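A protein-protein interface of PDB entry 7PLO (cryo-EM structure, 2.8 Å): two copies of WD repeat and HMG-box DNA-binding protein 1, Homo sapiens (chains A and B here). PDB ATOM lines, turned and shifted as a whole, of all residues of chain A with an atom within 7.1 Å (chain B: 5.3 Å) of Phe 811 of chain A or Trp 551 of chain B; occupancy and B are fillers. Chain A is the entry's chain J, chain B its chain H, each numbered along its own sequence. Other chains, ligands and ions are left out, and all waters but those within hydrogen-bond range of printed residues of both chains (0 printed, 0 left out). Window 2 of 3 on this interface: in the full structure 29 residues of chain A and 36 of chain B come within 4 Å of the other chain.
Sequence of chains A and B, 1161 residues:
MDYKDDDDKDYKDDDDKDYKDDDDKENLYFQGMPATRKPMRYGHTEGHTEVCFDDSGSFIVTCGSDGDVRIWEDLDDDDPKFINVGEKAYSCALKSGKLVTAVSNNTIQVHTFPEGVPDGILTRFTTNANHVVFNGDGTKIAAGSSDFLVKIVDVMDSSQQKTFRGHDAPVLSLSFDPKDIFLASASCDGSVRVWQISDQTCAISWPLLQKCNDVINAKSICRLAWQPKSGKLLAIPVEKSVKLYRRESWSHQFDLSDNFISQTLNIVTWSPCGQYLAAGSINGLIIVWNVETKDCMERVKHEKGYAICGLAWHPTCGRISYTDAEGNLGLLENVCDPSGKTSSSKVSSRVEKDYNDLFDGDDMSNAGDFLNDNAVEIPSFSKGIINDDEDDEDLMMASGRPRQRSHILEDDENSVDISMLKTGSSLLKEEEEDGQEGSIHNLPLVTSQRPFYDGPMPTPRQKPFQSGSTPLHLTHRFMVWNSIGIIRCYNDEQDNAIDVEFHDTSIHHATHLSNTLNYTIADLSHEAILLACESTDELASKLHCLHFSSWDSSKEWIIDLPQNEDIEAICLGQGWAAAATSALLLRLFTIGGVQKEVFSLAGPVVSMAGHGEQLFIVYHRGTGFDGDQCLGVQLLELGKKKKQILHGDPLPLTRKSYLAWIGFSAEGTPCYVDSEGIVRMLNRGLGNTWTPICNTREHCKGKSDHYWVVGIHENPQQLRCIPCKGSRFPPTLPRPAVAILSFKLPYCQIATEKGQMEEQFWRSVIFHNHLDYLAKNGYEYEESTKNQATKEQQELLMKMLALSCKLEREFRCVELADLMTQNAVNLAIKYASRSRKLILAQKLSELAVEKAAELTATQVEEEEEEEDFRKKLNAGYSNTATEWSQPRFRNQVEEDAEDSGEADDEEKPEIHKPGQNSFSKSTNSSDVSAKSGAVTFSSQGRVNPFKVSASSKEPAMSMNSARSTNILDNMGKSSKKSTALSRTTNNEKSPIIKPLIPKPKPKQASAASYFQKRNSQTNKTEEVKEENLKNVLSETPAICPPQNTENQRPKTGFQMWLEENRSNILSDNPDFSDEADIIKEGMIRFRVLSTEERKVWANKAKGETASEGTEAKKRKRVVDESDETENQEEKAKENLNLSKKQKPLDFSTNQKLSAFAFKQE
NE1 of Trp 551 of chain B sits at hydrogen-bond distance from OE1 of Glu 810 of chain A, 2.7 Å away. O of Gly 592 of chain B sits at hydrogen-bond distance from NH2 of Arg 812 of chain A, 2.9 Å away. OE2 of Glu 815 of chain A sits at hydrogen-bond distance from N of Gly 592 of chain B, 3.3 Å away.
OG of Ser 550 of chain B sits at hydrogen-bond distance from OD1 of Asp 552 of chain B, 2.8 Å away. The side-chain hydroxyl (OG) of Ser 550 of chain B sits at hydrogen-bond distance from the side-chain hydroxyl (OG) of Ser 554 of chain B (2.9 Å). OD1 of Asp 552 of chain B lies within hydrogen-bond range of OG of Ser 554 of chain B, at 2.8 Å. The backbone NH of Arg 809 of chain A sits at hydrogen-bond distance from the backbone carbonyl oxygen of Ser 804 of chain A (3.2 Å). O of Arg 809 of chain A is in hydrogen-bond range of SG of Cys 813 of chain A (3.4 Å).
Among the printed residues, merely in contact across the chains: Phe 811 of chain A with Ser 550 of chain B (3.3 Å), Phe 811 of chain A with Trp 551 of chain B (3.5 Å), Phe 811 of chain A with His 547 of chain B (3.6 Å), Ile 839 of chain A with Trp 551 of chain B (3.6 Å), Phe 811 of chain A with Ser 554 of chain B (3.8 Å) and Arg 809 of chain A with Ser 554 of chain B (3.9 Å).
Of chain B, only His 547, Ser 550, Trp 551 and Ser 554 come within 4 Å of Phe 811 of chain A. Of chain A, only Glu 810 (2.7 Å), Phe 811 (3.5 Å) and Ile 839 (3.6 Å) come within 4 Å of Trp 551 of chain B. Of the printed residues of chain B, Ile 839 of chain A touches Trp 551. Printed residues of chain B within 4 Å of Glu 810 of chain A: Trp 551 (2.7 Å). Printed residues of chain A within 4 Å of Gly 592 of chain B: Arg 812 and Glu 815. Of the printed residues of chain B, Glu 815 of chain A touches Gly 592. Of the printed residues of chain A, Ser 554 of chain B touches Arg 809 and Phe 811. Val 814 of chain A touches none of the printed residues of chain B. Ala 817 of chain A touches none of the printed residues of chain B. The nearest residue of chain B that does not touch Phe 811 of chain A is Asp 552 of chain B (4.2 Å).
Printed residues of chain B that touch a printed residue of chain A: His 547, Ser 550, Trp 551, Ser 554 and Gly 592. Hydrophobic or aromatic side chains of chain B that line the printed part of chain A: His 547 and Trp 551. Printed residues of chain A that touch a printed residue of chain B: Arg 809, Glu 810, Phe 811, Arg 812, Glu 815 and Ile 839. Hydrophobic or aromatic side chains of chain A within 4 Å of the printed part of chain B: Phe 811 and Ile 839. Among the printed residues, 9 pairs touch across the chains.
No position is printed for both chains.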
ATOM      1  N   SER A 804      24.386 -30.209 -21.316  1.00  0.00           N
ATOM      2  CA  SER A 804      24.655 -28.773 -21.279  1.00  0.00           C
ATOM      3  C   SER A 804      24.041 -28.128 -20.040  1.00  0.00           C
ATOM      4  O   SER A 804      24.655 -27.257 -19.414  1.00  0.00           O
ATOM      5  CB  SER A 804      24.121 -28.108 -22.547  1.00  0.00           C
ATOM      6  OG  SER A 804      24.695 -28.686 -23.707  1.00  0.00           O
ATOM      7  N   GLU A 808      25.536 -26.172 -16.887  1.00  0.00           N
ATOM      8  CA  GLU A 808      24.991 -24.822 -16.641  1.00  0.00           C
ATOM      9  C   GLU A 808      25.441 -23.804 -17.693  1.00  0.00           C
ATOM     10  O   GLU A 808      25.769 -22.656 -17.381  1.00  0.00           O
ATOM     11  CB  GLU A 808      25.282 -24.329 -15.204  1.00  0.00           C
ATOM     12  CG  GLU A 808      26.703 -24.454 -14.613  1.00  0.00           C
ATOM     13  CD  GLU A 808      27.702 -23.467 -15.188  1.00  0.00           C
ATOM     14  OE1 GLU A 808      27.367 -22.269 -15.295  1.00  0.00           O
ATOM     15  OE2 GLU A 808      28.831 -23.887 -15.516  1.00  0.00           O
ATOM     16  N   ARG A 809      25.414 -24.220 -18.961  1.00  0.00           N
ATOM     17  CA  ARG A 809      25.619 -23.325 -20.105  1.00  0.00           C
ATOM     18  C   ARG A 809      24.251 -23.039 -20.722  1.00  0.00           C
ATOM     19  O   ARG A 809      23.792 -23.740 -21.627  1.00  0.00           O
ATOM     20  CB  ARG A 809      26.596 -23.931 -21.105  1.00  0.00           C
ATOM     21  CG  ARG A 809      28.051 -23.781 -20.675  1.00  0.00           C
ATOM     22  CD  ARG A 809      29.028 -24.358 -21.689  1.00  0.00           C
ATOM     23  NE  ARG A 809      30.414 -24.204 -21.247  1.00  0.00           N
ATOM     24  CZ  ARG A 809      31.195 -23.155 -21.485  1.00  0.00           C
ATOM     25  NH1 ARG A 809      30.780 -22.114 -22.196  1.00  0.00           N
ATOM     26  NH2 ARG A 809      32.431 -23.146 -20.994  1.00  0.00           N
ATOM     27  N   GLU A 810      23.603 -21.983 -20.218  1.00  0.00           N
ATOM     28  CA  GLU A 810      22.264 -21.619 -20.674  1.00  0.00           C
ATOM     29  C   GLU A 810      22.262 -21.250 -22.153  1.00  0.00           C
ATOM     30  O   GLU A 810      21.299 -21.545 -22.874  1.00  0.00           O
ATOM     31  CB  GLU A 810      21.733 -20.465 -19.817  1.00  0.00           C
ATOM     32  CG  GLU A 810      20.455 -19.769 -20.330  1.00  0.00           C
ATOM     33  CD  GLU A 810      20.716 -18.543 -21.205  1.00  0.00           C
ATOM     34  OE1 GLU A 810      21.723 -17.833 -20.995  1.00  0.00           O
ATOM     35  OE2 GLU A 810      19.895 -18.286 -22.110  1.00  0.00           O
ATOM     36  N   PHE A 811      23.323 -20.583 -22.616  1.00  0.00           N
ATOM     37  CA  PHE A 811      23.427 -20.258 -24.035  1.00  0.00           C
ATOM     38  C   PHE A 811      23.459 -21.522 -24.885  1.00  0.00           C
ATOM     39  O   PHE A 811      22.778 -21.604 -25.913  1.00  0.00           O
ATOM     40  CB  PHE A 811      24.672 -19.411 -24.290  1.00  0.00           C
ATOM     41  CG  PHE A 811      24.493 -17.957 -23.967  1.00  0.00           C
ATOM     42  CD1 PHE A 811      23.937 -17.094 -24.897  1.00  0.00           C
ATOM     43  CD2 PHE A 811      24.881 -17.449 -22.737  1.00  0.00           C
ATOM     44  CE1 PHE A 811      23.769 -15.754 -24.607  1.00  0.00           C
ATOM     45  CE2 PHE A 811      24.715 -16.109 -22.443  1.00  0.00           C
ATOM     46  CZ  PHE A 811      24.159 -15.260 -23.379  1.00  0.00           C
ATOM     47  N   ARG A 812      24.230 -22.525 -24.458  1.00  0.00           N
ATOM     48  CA  ARG A 812      24.267 -23.790 -25.184  1.00  0.00           C
ATOM     49  C   ARG A 812      22.910 -24.480 -25.153  1.00  0.00           C
ATOM     50  O   ARG A 812      22.480 -25.069 -26.155  1.00  0.00           O
ATOM     51  CB  ARG A 812      25.346 -24.697 -24.592  1.00  0.00           C
ATOM     52  CG  ARG A 812      25.573 -25.974 -25.383  1.00  0.00           C
ATOM     53  CD  ARG A 812      26.770 -26.765 -24.883  1.00  0.00           C
ATOM     54  NE  ARG A 812      28.033 -26.065 -25.092  1.00  0.00           N
ATOM     55  CZ  ARG A 812      29.233 -26.553 -24.797  1.00  0.00           C
ATOM     56  NH1 ARG A 812      29.389 -27.762 -24.277  1.00  0.00           N
ATOM     57  NH2 ARG A 812      30.310 -25.807 -25.031  1.00  0.00           N
ATOM     58  N   CYS A 813      22.223 -24.423 -24.008  1.00  0.00           N
ATOM     59  CA  CYS A 813      20.907 -25.047 -23.904  1.00  0.00           C
ATOM     60  C   CYS A 813      19.913 -24.405 -24.865  1.00  0.00           C
ATOM     61  O   CYS A 813      19.155 -25.108 -25.542  1.00  0.00           O
ATOM     62  CB  CYS A 813      20.395 -24.958 -22.467  1.00  0.00           C
ATOM     63  SG  CYS A 813      21.251 -26.043 -21.299  1.00  0.00           S
ATOM     64  N   VAL A 814      19.911 -23.074 -24.953  1.00  0.00           N
ATOM     65  CA  VAL A 814      18.997 -22.397 -25.872  1.00  0.00           C
ATOM     66  C   VAL A 814      19.394 -22.674 -27.320  1.00  0.00           C
ATOM     67  O   VAL A 814      18.531 -22.845 -28.194  1.00  0.00           O
ATOM     68  CB  VAL A 814      18.952 -20.887 -25.562  1.00  0.00           C
ATOM     69  CG1 VAL A 814      18.191 -20.108 -26.656  1.00  0.00           C
ATOM     70  CG2 VAL A 814      18.320 -20.649 -24.183  1.00  0.00           C
ATOM     71  N   GLU A 815      20.701 -22.718 -27.599  1.00  0.00           N
ATOM     72  CA  GLU A 815      21.163 -22.994 -28.955  1.00  0.00           C
ATOM     73  C   GLU A 815      20.734 -24.383 -29.411  1.00  0.00           C
ATOM     74  O   GLU A 815      20.393 -24.583 -30.582  1.00  0.00           O
ATOM     75  CB  GLU A 815      22.685 -22.848 -29.023  1.00  0.00           C
ATOM     76  CG  GLU A 815      23.169 -21.401 -29.007  1.00  0.00           C
ATOM     77  CD  GLU A 815      24.657 -21.275 -28.724  1.00  0.00           C
ATOM     78  OE1 GLU A 815      25.345 -22.313 -28.626  1.00  0.00           O
ATOM     79  OE2 GLU A 815      25.141 -20.129 -28.599  1.00  0.00           O
ATOM     80  N   LEU A 816      20.745 -25.355 -28.497  1.00  0.00           N
ATOM     81  CA  LEU A 816      20.260 -26.690 -28.838  1.00  0.00           C
ATOM     82  C   LEU A 816      18.739 -26.722 -28.934  1.00  0.00           C
ATOM     83  O   LEU A 816      18.181 -27.392 -29.812  1.00  0.00           O
ATOM     84  CB  LEU A 816      20.753 -27.704 -27.806  1.00  0.00           C
ATOM     85  CG  LEU A 816      22.266 -27.935 -27.755  1.00  0.00           C
ATOM     86  CD1 LEU A 816      22.646 -28.663 -26.478  1.00  0.00           C
ATOM     87  CD2 LEU A 816      22.745 -28.716 -28.971  1.00  0.00           C
ATOM     88  N   ALA A 817      18.047 -26.004 -28.044  1.00  0.00           N
ATOM     89  CA  ALA A 817      16.588 -25.997 -28.049  1.00  0.00           C
ATOM     90  C   ALA A 817      16.005 -25.276 -29.257  1.00  0.00           C
ATOM     91  O   ALA A 817      14.817 -25.456 -29.549  1.00  0.00           O
ATOM     92  CB  ALA A 817      16.065 -25.347 -26.767  1.00  0.00           C
ATOM     93  N   ILE A 839      16.429 -18.786 -14.695  1.00  0.00           N
ATOM     94  CA  ILE A 839      16.627 -17.960 -15.883  1.00  0.00           C
ATOM     95  C   ILE A 839      16.616 -18.826 -17.138  1.00  0.00           C
ATOM     96  O   ILE A 839      16.067 -18.430 -18.175  1.00  0.00           O
ATOM     97  CB  ILE A 839      17.931 -17.142 -15.765  1.00  0.00           C
ATOM     98  CG1 ILE A 839      17.921 -16.244 -14.511  1.00  0.00           C
ATOM     99  CG2 ILE A 839      18.170 -16.300 -17.027  1.00  0.00           C
ATOM    100  CD1 ILE A 839      16.793 -15.202 -14.443  1.00  0.00           C
ATOM    101  N   LEU A 840      17.226 -20.011 -17.069  1.00  0.00           N
ATOM    102  CA  LEU A 840      17.187 -20.927 -18.203  1.00  0.00           C
ATOM    103  C   LEU A 840      15.759 -21.358 -18.509  1.00  0.00           C
ATOM    104  O   LEU A 840      15.355 -21.403 -19.677  1.00  0.00           O
ATOM    105  CB  LEU A 840      18.077 -22.141 -17.924  1.00  0.00           C
ATOM    106  CG  LEU A 840      18.055 -23.325 -18.900  1.00  0.00           C
ATOM    107  CD1 LEU A 840      18.352 -22.911 -20.335  1.00  0.00           C
ATOM    108  CD2 LEU A 840      19.051 -24.378 -18.443  1.00  0.00           C
ATOM    109  N   LYS A 843      13.923 -18.337 -20.141  1.00  0.00           N
ATOM    110  CA  LYS A 843      14.300 -18.049 -21.519  1.00  0.00           C
ATOM    111  C   LYS A 843      13.896 -19.178 -22.462  1.00  0.00           C
ATOM    112  O   LYS A 843      13.565 -18.918 -23.623  1.00  0.00           O
ATOM    113  CB  LYS A 843      15.798 -17.757 -21.594  1.00  0.00           C
ATOM    114  CG  LYS A 843      16.135 -16.379 -21.033  1.00  0.00           C
ATOM    115  CD  LYS A 843      17.621 -16.069 -21.056  1.00  0.00           C
ATOM    116  CE  LYS A 843      17.897 -14.674 -20.503  1.00  0.00           C
ATOM    117  NZ  LYS A 843      17.386 -13.592 -21.393  1.00  0.00           N
ATOM    118  N   HIS B 547      33.321 -15.328 -24.956  1.00  0.00           N
ATOM    119  CA  HIS B 547      31.957 -14.804 -24.951  1.00  0.00           C
ATOM    120  C   HIS B 547      31.827 -13.699 -23.896  1.00  0.00           C
ATOM    121  O   HIS B 547      31.109 -13.822 -22.903  1.00  0.00           O
ATOM    122  CB  HIS B 547      30.982 -15.949 -24.698  1.00  0.00           C
ATOM    123  CG  HIS B 547      29.539 -15.596 -24.888  1.00  0.00           C
ATOM    124  ND1 HIS B 547      29.120 -14.431 -25.494  1.00  0.00           N
ATOM    125  CD2 HIS B 547      28.413 -16.272 -24.559  1.00  0.00           C
ATOM    126  CE1 HIS B 547      27.800 -14.401 -25.522  1.00  0.00           C
ATOM    127  NE2 HIS B 547      27.346 -15.506 -24.959  1.00  0.00           N
ATOM    128  N   SER B 549      30.397 -10.860 -23.916  1.00  0.00           N
ATOM    129  CA  SER B 549      29.101 -10.202 -23.797  1.00  0.00           C
ATOM    130  C   SER B 549      28.090 -10.988 -22.966  1.00  0.00           C
ATOM    131  O   SER B 549      26.946 -10.541 -22.836  1.00  0.00           O
ATOM    132  CB  SER B 549      28.520  -9.948 -25.192  1.00  0.00           C
ATOM    133  OG  SER B 549      29.420  -9.198 -25.990  1.00  0.00           O
ATOM    134  N   SER B 550      28.472 -12.134 -22.405  1.00  0.00           N
ATOM    135  CA  SER B 550      27.540 -12.970 -21.667  1.00  0.00           C
ATOM    136  C   SER B 550      27.078 -12.290 -20.382  1.00  0.00           C
ATOM    137  O   SER B 550      27.740 -11.403 -19.835  1.00  0.00           O
ATOM    138  CB  SER B 550      28.185 -14.310 -21.327  1.00  0.00           C
ATOM    139  OG  SER B 550      27.276 -15.141 -20.633  1.00  0.00           O
ATOM    140  N   TRP B 551      25.917 -12.734 -19.901  1.00  0.00           N
ATOM    141  CA  TRP B 551      25.339 -12.265 -18.647  1.00  0.00           C
ATOM    142  C   TRP B 551      25.795 -13.065 -17.430  1.00  0.00           C
ATOM    143  O   TRP B 551      25.451 -12.685 -16.305  1.00  0.00           O
ATOM    144  CB  TRP B 551      23.806 -12.308 -18.726  1.00  0.00           C
ATOM    145  CG  TRP B 551      23.232 -13.702 -18.761  1.00  0.00           C
ATOM    146  CD1 TRP B 551      23.083 -14.501 -19.859  1.00  0.00           C
ATOM    147  CD2 TRP B 551      22.725 -14.453 -17.649  1.00  0.00           C
ATOM    148  NE1 TRP B 551      22.523 -15.703 -19.499  1.00  0.00           N
ATOM    149  CE2 TRP B 551      22.292 -15.698 -18.148  1.00  0.00           C
ATOM    150  CE3 TRP B 551      22.598 -14.193 -16.281  1.00  0.00           C
ATOM    151  CZ2 TRP B 551      21.742 -16.681 -17.328  1.00  0.00           C
ATOM    152  CZ3 TRP B 551      22.052 -15.172 -15.468  1.00  0.00           C
ATOM    153  CH2 TRP B 551      21.630 -16.399 -15.995  1.00  0.00           C
ATOM    154  N   ASP B 552      26.553 -14.143 -17.614  1.00  0.00           N
ATOM    155  CA  ASP B 552      26.949 -15.020 -16.513  1.00  0.00           C
ATOM    156  C   ASP B 552      28.342 -15.569 -16.823  1.00  0.00           C
ATOM    157  O   ASP B 552      29.049 -15.043 -17.689  1.00  0.00           O
ATOM    158  CB  ASP B 552      25.882 -16.111 -16.294  1.00  0.00           C
ATOM    159  CG  ASP B 552      25.707 -17.018 -17.500  1.00  0.00           C
ATOM    160  OD1 ASP B 552      26.219 -16.685 -18.590  1.00  0.00           O
ATOM    161  OD2 ASP B 552      25.053 -18.071 -17.354  1.00  0.00           O
ATOM    162  N   SER B 553      28.735 -16.642 -16.128  1.00  0.00           N
ATOM    163  CA  SER B 553      30.108 -17.137 -16.122  1.00  0.00           C
ATOM    164  C   SER B 553      30.403 -18.115 -17.260  1.00  0.00           C
ATOM    165  O   SER B 553      31.281 -18.976 -17.115  1.00  0.00           O
ATOM    166  CB  SER B 553      30.414 -17.789 -14.772  1.00  0.00           C
ATOM    167  OG  SER B 553      29.571 -18.905 -14.548  1.00  0.00           O
ATOM    168  N   SER B 554      29.701 -18.001 -18.391  1.00  0.00           N
ATOM    169  CA  SER B 554      29.972 -18.788 -19.590  1.00  0.00           C
ATOM    170  C   SER B 554      30.938 -18.075 -20.534  1.00  0.00           C
ATOM    171  O   SER B 554      30.833 -18.209 -21.761  1.00  0.00           O
ATOM    172  CB  SER B 554      28.657 -19.115 -20.302  1.00  0.00           C
ATOM    173  OG  SER B 554      27.889 -17.944 -20.512  1.00  0.00           O
ATOM    174  N   GLY B 592      28.422 -20.686 -28.395  1.00  0.00           N
ATOM    175  CA  GLY B 592      28.275 -21.527 -27.220  1.00  0.00           C
ATOM    176  C   GLY B 592      28.950 -22.884 -27.318  1.00  0.00           C
ATOM    177  O   GLY B 592      28.971 -23.611 -26.320  1.00  0.00           O
